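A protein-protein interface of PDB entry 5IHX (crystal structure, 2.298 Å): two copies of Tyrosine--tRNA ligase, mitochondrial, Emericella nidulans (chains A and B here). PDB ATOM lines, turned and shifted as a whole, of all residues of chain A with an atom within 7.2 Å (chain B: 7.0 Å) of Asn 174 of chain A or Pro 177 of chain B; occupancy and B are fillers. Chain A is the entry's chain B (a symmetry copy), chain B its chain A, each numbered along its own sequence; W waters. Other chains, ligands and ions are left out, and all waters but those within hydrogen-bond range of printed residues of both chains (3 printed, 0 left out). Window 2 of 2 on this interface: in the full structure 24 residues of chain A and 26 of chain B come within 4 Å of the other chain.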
ATOM      1  N   ALA A 107     -14.685  17.445  12.981  1.00  0.00           N
ATOM      2  CA  ALA A 107     -14.678  16.642  14.203  1.00  0.00           C
ATOM      3  C   ALA A 107     -13.513  15.671  14.210  1.00  0.00           C
ATOM      4  O   ALA A 107     -12.747  15.598  15.170  1.00  0.00           O
ATOM      5  CB  ALA A 107     -15.986  15.868  14.337  1.00  0.00           C
ATOM      6  N   ASN A 169     -18.690  17.802   9.328  1.00  0.00           N
ATOM      7  CA  ASN A 169     -19.232  16.614   9.983  1.00  0.00           C
ATOM      8  C   ASN A 169     -19.412  16.815  11.488  1.00  0.00           C
ATOM      9  O   ASN A 169     -19.976  15.959  12.169  1.00  0.00           O
ATOM     10  CB  ASN A 169     -18.357  15.384   9.713  1.00  0.00           C
ATOM     11  CG  ASN A 169     -16.959  15.503  10.292  1.00  0.00           C
ATOM     12  OD1 ASN A 169     -16.632  16.458  10.995  1.00  0.00           O
ATOM     13  ND2 ASN A 169     -16.130  14.506  10.014  1.00  0.00           N
ATOM     14  N   ASN A 170     -18.938  17.950  11.995  1.00  0.00           N
ATOM     15  CA  ASN A 170     -19.262  18.385  13.351  1.00  0.00           C
ATOM     16  C   ASN A 170     -20.767  18.504  13.541  1.00  0.00           C
ATOM     17  O   ASN A 170     -21.268  18.417  14.661  1.00  0.00           O
ATOM     18  CB  ASN A 170     -18.594  19.729  13.666  1.00  0.00           C
ATOM     19  CG  ASN A 170     -17.229  19.575  14.313  1.00  0.00           C
ATOM     20  OD1 ASN A 170     -16.992  18.645  15.084  1.00  0.00           O
ATOM     21  ND2 ASN A 170     -16.321  20.491  14.000  1.00  0.00           N
ATOM     22  N   VAL A 171     -21.478  18.718  12.438  1.00  0.00           N
ATOM     23  CA  VAL A 171     -22.931  18.848  12.459  1.00  0.00           C
ATOM     24  C   VAL A 171     -23.595  17.667  13.167  1.00  0.00           C
ATOM     25  O   VAL A 171     -24.582  17.857  13.874  1.00  0.00           O
ATOM     26  CB  VAL A 171     -23.494  18.990  11.019  1.00  0.00           C
ATOM     27  CG1 VAL A 171     -24.993  18.696  10.969  1.00  0.00           C
ATOM     28  CG2 VAL A 171     -23.209  20.381  10.477  1.00  0.00           C
ATOM     29  N   TRP A 172     -23.062  16.460  12.980  1.00  0.00           N
ATOM     30  CA  TRP A 172     -23.583  15.287  13.684  1.00  0.00           C
ATOM     31  C   TRP A 172     -22.656  14.802  14.806  1.00  0.00           C
ATOM     32  O   TRP A 172     -23.136  14.342  15.844  1.00  0.00           O
ATOM     33  CB  TRP A 172     -23.880  14.134  12.708  1.00  0.00           C
ATOM     34  CG  TRP A 172     -22.819  13.790  11.698  1.00  0.00           C
ATOM     35  CD1 TRP A 172     -21.748  12.962  11.880  1.00  0.00           C
ATOM     36  CD2 TRP A 172     -22.760  14.231  10.334  1.00  0.00           C
ATOM     37  NE1 TRP A 172     -21.018  12.873  10.716  1.00  0.00           N
ATOM     38  CE2 TRP A 172     -21.618  13.641   9.753  1.00  0.00           C
ATOM     39  CE3 TRP A 172     -23.557  15.072   9.551  1.00  0.00           C
ATOM     40  CZ2 TRP A 172     -21.252  13.872   8.428  1.00  0.00           C
ATOM     41  CZ3 TRP A 172     -23.190  15.298   8.236  1.00  0.00           C
ATOM     42  CH2 TRP A 172     -22.049  14.699   7.688  1.00  0.00           C
ATOM     43  N   TRP A 173     -21.344  14.901  14.621  1.00  0.00           N
ATOM     44  CA  TRP A 173     -20.412  14.371  15.621  1.00  0.00           C
ATOM     45  C   TRP A 173     -20.487  15.110  16.959  1.00  0.00           C
ATOM     46  O   TRP A 173     -20.001  14.610  17.973  1.00  0.00           O
ATOM     47  CB  TRP A 173     -18.977  14.399  15.094  1.00  0.00           C
ATOM     48  CG  TRP A 173     -18.702  13.314  14.100  1.00  0.00           C
ATOM     49  CD1 TRP A 173     -18.213  13.460  12.834  1.00  0.00           C
ATOM     50  CD2 TRP A 173     -18.913  11.909  14.286  1.00  0.00           C
ATOM     51  NE1 TRP A 173     -18.101  12.235  12.224  1.00  0.00           N
ATOM     52  CE2 TRP A 173     -18.526  11.266  13.095  1.00  0.00           C
ATOM     53  CE3 TRP A 173     -19.390  11.133  15.348  1.00  0.00           C
ATOM     54  CZ2 TRP A 173     -18.605   9.884  12.934  1.00  0.00           C
ATOM     55  CZ3 TRP A 173     -19.468   9.764  15.186  1.00  0.00           C
ATOM     56  CH2 TRP A 173     -19.076   9.154  13.990  1.00  0.00           C
ATOM     57  N   ASN A 174     -21.083  16.297  16.966  1.00  0.00           N
ATOM     58  CA  ASN A 174     -21.262  17.040  18.209  1.00  0.00           C
ATOM     59  C   ASN A 174     -22.252  16.354  19.153  1.00  0.00           C
ATOM     60  O   ASN A 174     -22.181  16.541  20.364  1.00  0.00           O
ATOM     61  CB  ASN A 174     -21.731  18.468  17.917  1.00  0.00           C
ATOM     62  CG  ASN A 174     -20.592  19.386  17.490  1.00  0.00           C
ATOM     63  OD1 ASN A 174     -19.418  19.012  17.546  1.00  0.00           O
ATOM     64  ND2 ASN A 174     -20.938  20.597  17.063  1.00  0.00           N
ATOM     65  N   LYS A 175     -23.170  15.565  18.592  1.00  0.00           N
ATOM     66  CA  LYS A 175     -24.218  14.916  19.381  1.00  0.00           C
ATOM     67  C   LYS A 175     -24.282  13.397  19.214  1.00  0.00           C
ATOM     68  O   LYS A 175     -24.867  12.716  20.056  1.00  0.00           O
ATOM     69  CB  LYS A 175     -25.586  15.504  19.019  1.00  0.00           C
ATOM     70  CG  LYS A 175     -25.710  17.002  19.240  1.00  0.00           C
ATOM     71  CD  LYS A 175     -25.503  17.369  20.701  1.00  0.00           C
ATOM     72  N   THR A 176     -23.697  12.871  18.140  1.00  0.00           N
ATOM     73  CA  THR A 176     -23.828  11.448  17.811  1.00  0.00           C
ATOM     74  C   THR A 176     -23.414  10.541  18.972  1.00  0.00           C
ATOM     75  O   THR A 176     -22.227  10.457  19.300  1.00  0.00           O
ATOM     76  CB  THR A 176     -22.989  11.080  16.571  1.00  0.00           C
ATOM     77  OG1 THR A 176     -23.498  11.761  15.415  1.00  0.00           O
ATOM     78  CG2 THR A 176     -23.020   9.572  16.315  1.00  0.00           C
ATOM     79  N   PRO A 177     -24.391   9.847  19.589  1.00  0.00           N
ATOM     80  CA  PRO A 177     -24.067   8.969  20.721  1.00  0.00           C
ATOM     81  C   PRO A 177     -23.177   7.792  20.336  1.00  0.00           C
ATOM     82  O   PRO A 177     -23.357   7.207  19.269  1.00  0.00           O
ATOM     83  CB  PRO A 177     -25.442   8.461  21.183  1.00  0.00           C
ATOM     84  CG  PRO A 177     -26.423   9.426  20.638  1.00  0.00           C
ATOM     85  CD  PRO A 177     -25.843   9.889  19.340  1.00  0.00           C
ATOM     86  N   LEU A 178     -22.220   7.467  21.198  1.00  0.00           N
ATOM     87  CA  LEU A 178     -21.408   6.270  21.024  1.00  0.00           C
ATOM     88  C   LEU A 178     -22.301   5.047  20.847  1.00  0.00           C
ATOM     89  O   LEU A 178     -22.036   4.191  20.002  1.00  0.00           O
ATOM     90  CB  LEU A 178     -20.472   6.082  22.223  1.00  0.00           C
ATOM     91  CG  LEU A 178     -19.801   4.716  22.405  1.00  0.00           C
ATOM     92  CD1 LEU A 178     -19.061   4.264  21.159  1.00  0.00           C
ATOM     93  CD2 LEU A 178     -18.841   4.778  23.579  1.00  0.00           C
ATOM     94  N   LEU A 179     -23.378   4.989  21.624  1.00  0.00           N
ATOM     95  CA  LEU A 179     -24.267   3.832  21.612  1.00  0.00           C
ATOM     96  C   LEU A 179     -24.918   3.632  20.245  1.00  0.00           C
ATOM     97  O   LEU A 179     -25.119   2.498  19.810  1.00  0.00           O
ATOM     98  CB  LEU A 179     -25.342   3.982  22.691  1.00  0.00           C
ATOM     99  CG  LEU A 179     -26.083   2.716  23.133  1.00  0.00           C
ATOM    100  CD1 LEU A 179     -25.129   1.632  23.616  1.00  0.00           C
ATOM    101  CD2 LEU A 179     -27.092   3.052  24.221  1.00  0.00           C
ATOM    102  N   TRP B 172     -26.613   8.372  31.071  1.00  0.00           N
ATOM    103  CA  TRP B 172     -25.608   9.067  30.272  1.00  0.00           C
ATOM    104  C   TRP B 172     -25.410   8.445  28.887  1.00  0.00           C
ATOM    105  O   TRP B 172     -25.200   9.171  27.917  1.00  0.00           O
ATOM    106  CB  TRP B 172     -24.264   9.135  31.016  1.00  0.00           C
ATOM    107  CG  TRP B 172     -23.760   7.858  31.635  1.00  0.00           C
ATOM    108  CD1 TRP B 172     -23.046   6.871  31.017  1.00  0.00           C
ATOM    109  CD2 TRP B 172     -23.885   7.460  33.009  1.00  0.00           C
ATOM    110  NE1 TRP B 172     -22.736   5.876  31.915  1.00  0.00           N
ATOM    111  CE2 TRP B 172     -23.239   6.214  33.143  1.00  0.00           C
ATOM    112  CE3 TRP B 172     -24.489   8.032  34.133  1.00  0.00           C
ATOM    113  CZ2 TRP B 172     -23.185   5.530  34.356  1.00  0.00           C
ATOM    114  CZ3 TRP B 172     -24.433   7.350  35.335  1.00  0.00           C
ATOM    115  CH2 TRP B 172     -23.784   6.114  35.437  1.00  0.00           C
ATOM    116  N   TRP B 173     -25.485   7.122  28.776  1.00  0.00           N
ATOM    117  CA  TRP B 173     -25.203   6.475  27.491  1.00  0.00           C
ATOM    118  C   TRP B 173     -26.216   6.793  26.394  1.00  0.00           C
ATOM    119  O   TRP B 173     -25.928   6.606  25.213  1.00  0.00           O
ATOM    120  CB  TRP B 173     -25.116   4.956  27.660  1.00  0.00           C
ATOM    121  CG  TRP B 173     -23.839   4.508  28.288  1.00  0.00           C
ATOM    122  CD1 TRP B 173     -23.699   3.725  29.394  1.00  0.00           C
ATOM    123  CD2 TRP B 173     -22.514   4.828  27.850  1.00  0.00           C
ATOM    124  NE1 TRP B 173     -22.367   3.531  29.670  1.00  0.00           N
ATOM    125  CE2 TRP B 173     -21.620   4.202  28.738  1.00  0.00           C
ATOM    126  CE3 TRP B 173     -21.998   5.585  26.794  1.00  0.00           C
ATOM    127  CZ2 TRP B 173     -20.238   4.309  28.602  1.00  0.00           C
ATOM    128  CZ3 TRP B 173     -20.629   5.692  26.661  1.00  0.00           C
ATOM    129  CH2 TRP B 173     -19.763   5.055  27.559  1.00  0.00           C
ATOM    130  N   ASN B 174     -27.395   7.271  26.771  1.00  0.00           N
ATOM    131  CA  ASN B 174     -28.397   7.635  25.779  1.00  0.00           C
ATOM    132  C   ASN B 174     -27.996   8.864  24.962  1.00  0.00           C
ATOM    133  O   ASN B 174     -28.432   9.018  23.823  1.00  0.00           O
ATOM    134  CB  ASN B 174     -29.750   7.877  26.451  1.00  0.00           C
ATOM    135  CG  ASN B 174     -30.476   6.583  26.793  1.00  0.00           C
ATOM    136  OD1 ASN B 174     -30.044   5.492  26.414  1.00  0.00           O
ATOM    137  ND2 ASN B 174     -31.596   6.703  27.497  1.00  0.00           N
ATOM    138  N   LYS B 175     -27.166   9.727  25.543  1.00  0.00           N
ATOM    139  CA  LYS B 175     -26.786  10.982  24.894  1.00  0.00           C
ATOM    140  C   LYS B 175     -25.273  11.183  24.746  1.00  0.00           C
ATOM    141  O   LYS B 175     -24.844  12.000  23.932  1.00  0.00           O
ATOM    142  CB  LYS B 175     -27.388  12.162  25.664  1.00  0.00           C
ATOM    143  CG  LYS B 175     -27.100  12.160  27.158  1.00  0.00           C
ATOM    144  CD  LYS B 175     -27.837  13.286  27.864  1.00  0.00           C
ATOM    145  N   THR B 176     -24.475  10.451  25.522  1.00  0.00           N
ATOM    146  CA  THR B 176     -23.022  10.647  25.538  1.00  0.00           C
ATOM    147  C   THR B 176     -22.404  10.538  24.138  1.00  0.00           C
ATOM    148  O   THR B 176     -22.372   9.450  23.561  1.00  0.00           O
ATOM    149  CB  THR B 176     -22.325   9.624  26.464  1.00  0.00           C
ATOM    150  OG1 THR B 176     -22.727   9.840  27.822  1.00  0.00           O
ATOM    151  CG2 THR B 176     -20.803   9.746  26.371  1.00  0.00           C
ATOM    152  N   PRO B 177     -21.903  11.663  23.590  1.00  0.00           N
ATOM    153  CA  PRO B 177     -21.312  11.616  22.245  1.00  0.00           C
ATOM    154  C   PRO B 177     -20.059  10.748  22.155  1.00  0.00           C
ATOM    155  O   PRO B 177     -19.233  10.738  23.072  1.00  0.00           O
ATOM    156  CB  PRO B 177     -20.966  13.085  21.959  1.00  0.00           C
ATOM    157  CG  PRO B 177     -21.808  13.878  22.886  1.00  0.00           C
ATOM    158  CD  PRO B 177     -21.936  13.039  24.116  1.00  0.00           C
ATOM    159  N   LEU B 178     -19.934  10.008  21.057  1.00  0.00           N
ATOM    160  CA  LEU B 178     -18.725   9.243  20.780  1.00  0.00           C
ATOM    161  C   LEU B 178     -17.489  10.132  20.868  1.00  0.00           C
ATOM    162  O   LEU B 178     -16.460   9.730  21.408  1.00  0.00           O
ATOM    163  CB  LEU B 178     -18.810   8.593  19.393  1.00  0.00           C
ATOM    164  CG  LEU B 178     -17.517   8.041  18.778  1.00  0.00           C
ATOM    165  CD1 LEU B 178     -16.816   7.069  19.707  1.00  0.00           C
ATOM    166  CD2 LEU B 178     -17.822   7.357  17.458  1.00  0.00           C
ATOM    167  N   LEU B 179     -17.605  11.352  20.359  1.00  0.00           N
ATOM    168  CA  LEU B 179     -16.464  12.258  20.304  1.00  0.00           C
ATOM    169  C   LEU B 179     -15.964  12.587  21.712  1.00  0.00           C
ATOM    170  O   LEU B 179     -14.761  12.729  21.932  1.00  0.00           O
ATOM    171  CB  LEU B 179     -16.834  13.538  19.550  1.00  0.00           C
ATOM    172  CG  LEU B 179     -15.686  14.374  18.977  1.00  0.00           C
ATOM    173  CD1 LEU B 179     -14.801  13.553  18.043  1.00  0.00           C
ATOM    174  CD2 LEU B 179     -16.226  15.595  18.250  1.00  0.00           C
ATOM    175  N   GLU B 180     -16.885  12.695  22.665  1.00  0.00           N
ATOM    176  CA  GLU B 180     -16.515  12.986  24.048  1.00  0.00           C
ATOM    177  C   GLU B 180     -15.688  11.855  24.660  1.00  0.00           C
ATOM    178  O   GLU B 180     -14.703  12.106  25.356  1.00  0.00           O
ATOM    179  CB  GLU B 180     -17.763  13.235  24.903  1.00  0.00           C
ATOM    180  CG  GLU B 180     -17.449  13.594  26.353  1.00  0.00           C
ATOM    181  CD  GLU B 180     -18.691  13.822  27.195  1.00  0.00           C
ATOM    182  OE1 GLU B 180     -19.812  13.748  26.650  1.00  0.00           O
ATOM    183  OE2 GLU B 180     -18.548  14.077  28.408  1.00  0.00           O
ATOM    184  N   VAL B 181     -16.085  10.612  24.405  1.00  0.00           N
ATOM    185  CA  VAL B 181     -15.364   9.466  24.954  1.00  0.00           C
ATOM    186  C   VAL B 181     -13.987   9.339  24.306  1.00  0.00           C
ATOM    187  O   VAL B 181     -13.003   9.014  24.974  1.00  0.00           O
ATOM    188  CB  VAL B 181     -16.158   8.154  24.773  1.00  0.00           C
ATOM    189  CG1 VAL B 181     -15.330   6.951  25.216  1.00  0.00           C
ATOM    190  CG2 VAL B 181     -17.467   8.212  25.549  1.00  0.00           C
ATOM    191  N   LEU B 182     -13.921   9.581  23.001  1.00  0.00           N
ATOM    192  CA  LEU B 182     -12.651   9.522  22.286  1.00  0.00           C
ATOM    193  C   LEU B 182     -11.702  10.618  22.762  1.00  0.00           C
ATOM    194  O   LEU B 182     -10.502  10.391  22.899  1.00  0.00           O
ATOM    195  CB  LEU B 182     -12.872   9.639  20.776  1.00  0.00           C
ATOM    196  CG  LEU B 182     -13.662   8.514  20.100  1.00  0.00           C
ATOM    197  CD1 LEU B 182     -13.664   8.695  18.589  1.00  0.00           C
ATOM    198  CD2 LEU B 182     -13.115   7.142  20.470  1.00  0.00           C
ATOM    199  N   TRP B 223     -15.976   4.236  31.682  1.00  0.00           N
ATOM    200  CA  TRP B 223     -16.680   5.509  31.656  1.00  0.00           C
ATOM    201  C   TRP B 223     -17.781   5.530  32.720  1.00  0.00           C
ATOM    202  O   TRP B 223     -17.984   6.547  33.384  1.00  0.00           O
ATOM    203  CB  TRP B 223     -17.259   5.777  30.263  1.00  0.00           C
ATOM    204  CG  TRP B 223     -17.706   7.194  30.065  1.00  0.00           C
ATOM    205  CD1 TRP B 223     -18.979   7.677  30.164  1.00  0.00           C
ATOM    206  CD2 TRP B 223     -16.875   8.315  29.743  1.00  0.00           C
ATOM    207  NE1 TRP B 223     -18.991   9.030  29.917  1.00  0.00           N
ATOM    208  CE2 TRP B 223     -17.712   9.446  29.659  1.00  0.00           C
ATOM    209  CE3 TRP B 223     -15.504   8.473  29.515  1.00  0.00           C
ATOM    210  CZ2 TRP B 223     -17.223  10.716  29.355  1.00  0.00           C
ATOM    211  CZ3 TRP B 223     -15.020   9.733  29.217  1.00  0.00           C
ATOM    212  CH2 TRP B 223     -15.878  10.838  29.139  1.00  0.00           C
HETATM  213  O   HOH W   1     -23.731   6.955  23.958  1.00  0.00           O
HETATM  214  O   HOH W   2     -20.090  12.036  18.704  1.00  0.00           O
HETATM  215  O   HOH W   3     -25.966  13.391  22.329  1.00  0.00           O
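The backbone carbonyl oxygen (O) of Thr 176 of chain B sits at hydrogen-bond distance from the backbone NH (N) of Leu 178 of chain A (3.1 Å). O of Thr 176 of chain A is in hydrogen-bond range of N of Leu 178 of chain B. N of Leu 178 of chain A sits close to N of Leu 178 of chain B, 3.4 Å away.
O of Trp 172 of chain B lies within hydrogen-bond range of OG1 of Thr 176 of chain B. N of Ala 107 of chain A sits at hydrogen-bond distance from OD1 of Asn 169 of chain A (3.0 Å). The backbone NH (N) of Ala 107 of chain A sits close to the side-chain amide oxygen (OD1) of Asn 170 of chain A, at 3.3 Å. ND2 of Asn 174 of chain A lies close to O of Asn 170 of chain A, at 3.3 Å. O of Trp 172 of chain A sits at hydrogen-bond distance from OG1 of Thr 176 of chain A (2.6 Å).
Ala 107 of chain A touches Leu 179 of chain B (CB to CD2, 3.9 Å). CZ3 of Trp 173 of chain A touches CD2 of Leu 178 of chain B, at 3.7 Å. CB of Leu 179 of chain B touches O of Trp 173 of chain A, at 3.7 Å. CG of Pro 177 of chain B touches O of Asn 174 of chain A (3.7 Å). Lys 175 of chain A touches Lys 175 of chain B. Thr 176 of chain A touches Pro 177 of chain B (O to CA, 3.3 Å). CA of Pro 177 of chain A touches O of Thr 176 of chain B (3.3 Å). Leu 178 of chain B touches Pro 177 of chain A (N to C, 3.99 Å). CD2 of Leu 178 of chain A touches CZ3 of Trp 173 of chain B, 3.7 Å away. Trp 173 of chain B touches Leu 179 of chain A.
Printed residues of chain A within 4 Å of Asn 174 of chain B: Pro 177 (3.8 Å). Of the printed residues of chain A, Leu 179 of chain B touches Ala 107 and Trp 173. Printed residues of chain B within 4 Å of Leu 179 of chain A: Trp 173. Leu 182 of chain B touches none of the printed residues of chain A. The nearest residue of chain B that does not touch Asn 174 of chain A is Leu 179 of chain B (4.7 Å).
Of the 12 printed residues of chain B, 7 touch a printed residue of chain A. Among the printed residues, no Asp or Glu carboxylate lies within 4 Å of a Lys or Arg side-chain nitrogen of the other chain.
Trp 173 of chain A touches Leu 178 of chain B, and with the chains exchanged Leu 178 of chain A touches Trp 173 of chain B. Asn 174 of chain A touches Pro 177 of chain B, and with the chains exchanged Pro 177 of chain A touches Asn 174 of chain B. Thr 176 of chain A touches Leu 178 of chain B, and with the chains exchanged Leu 178 of chain A touches Thr 176 of chain B. Pro 177 of chain A touches Leu 178 of chain B, but with the chains exchanged Leu 178 of chain A does not touch Pro 177 of chain B (4.04 Å). Positions printed for both chains: 172, 173, 174, 175, 176, 177, 178 and 179. Of the 14 pairs that touch across the chains among the printed residues, 12 have their exchanged pair printed and touching as well.
Water W3 bridges O of Lys 175 of chain B (2.4 Å) and O of Lys 175 of chain A (2.6 Å). Water W1 lies within hydrogen-bond range of the backbone carbonyl oxygen of Trp 173 of chain B, the backbone carbonyl oxygen of Thr 176 of chain B, the backbone NH of Leu 179 of chain A and the backbone NH of Leu 178 of chain A. Water W2 lies within hydrogen-bond range of the backbone carbonyl oxygen of Trp 173 of chain A (2.7 Å), the backbone carbonyl oxygen of Thr 176 of chain A (2.7 Å), the backbone NH of Leu 179 of chain B (3.1 Å) and the backbone NH of Leu 178 of chain B (3.1 Å).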
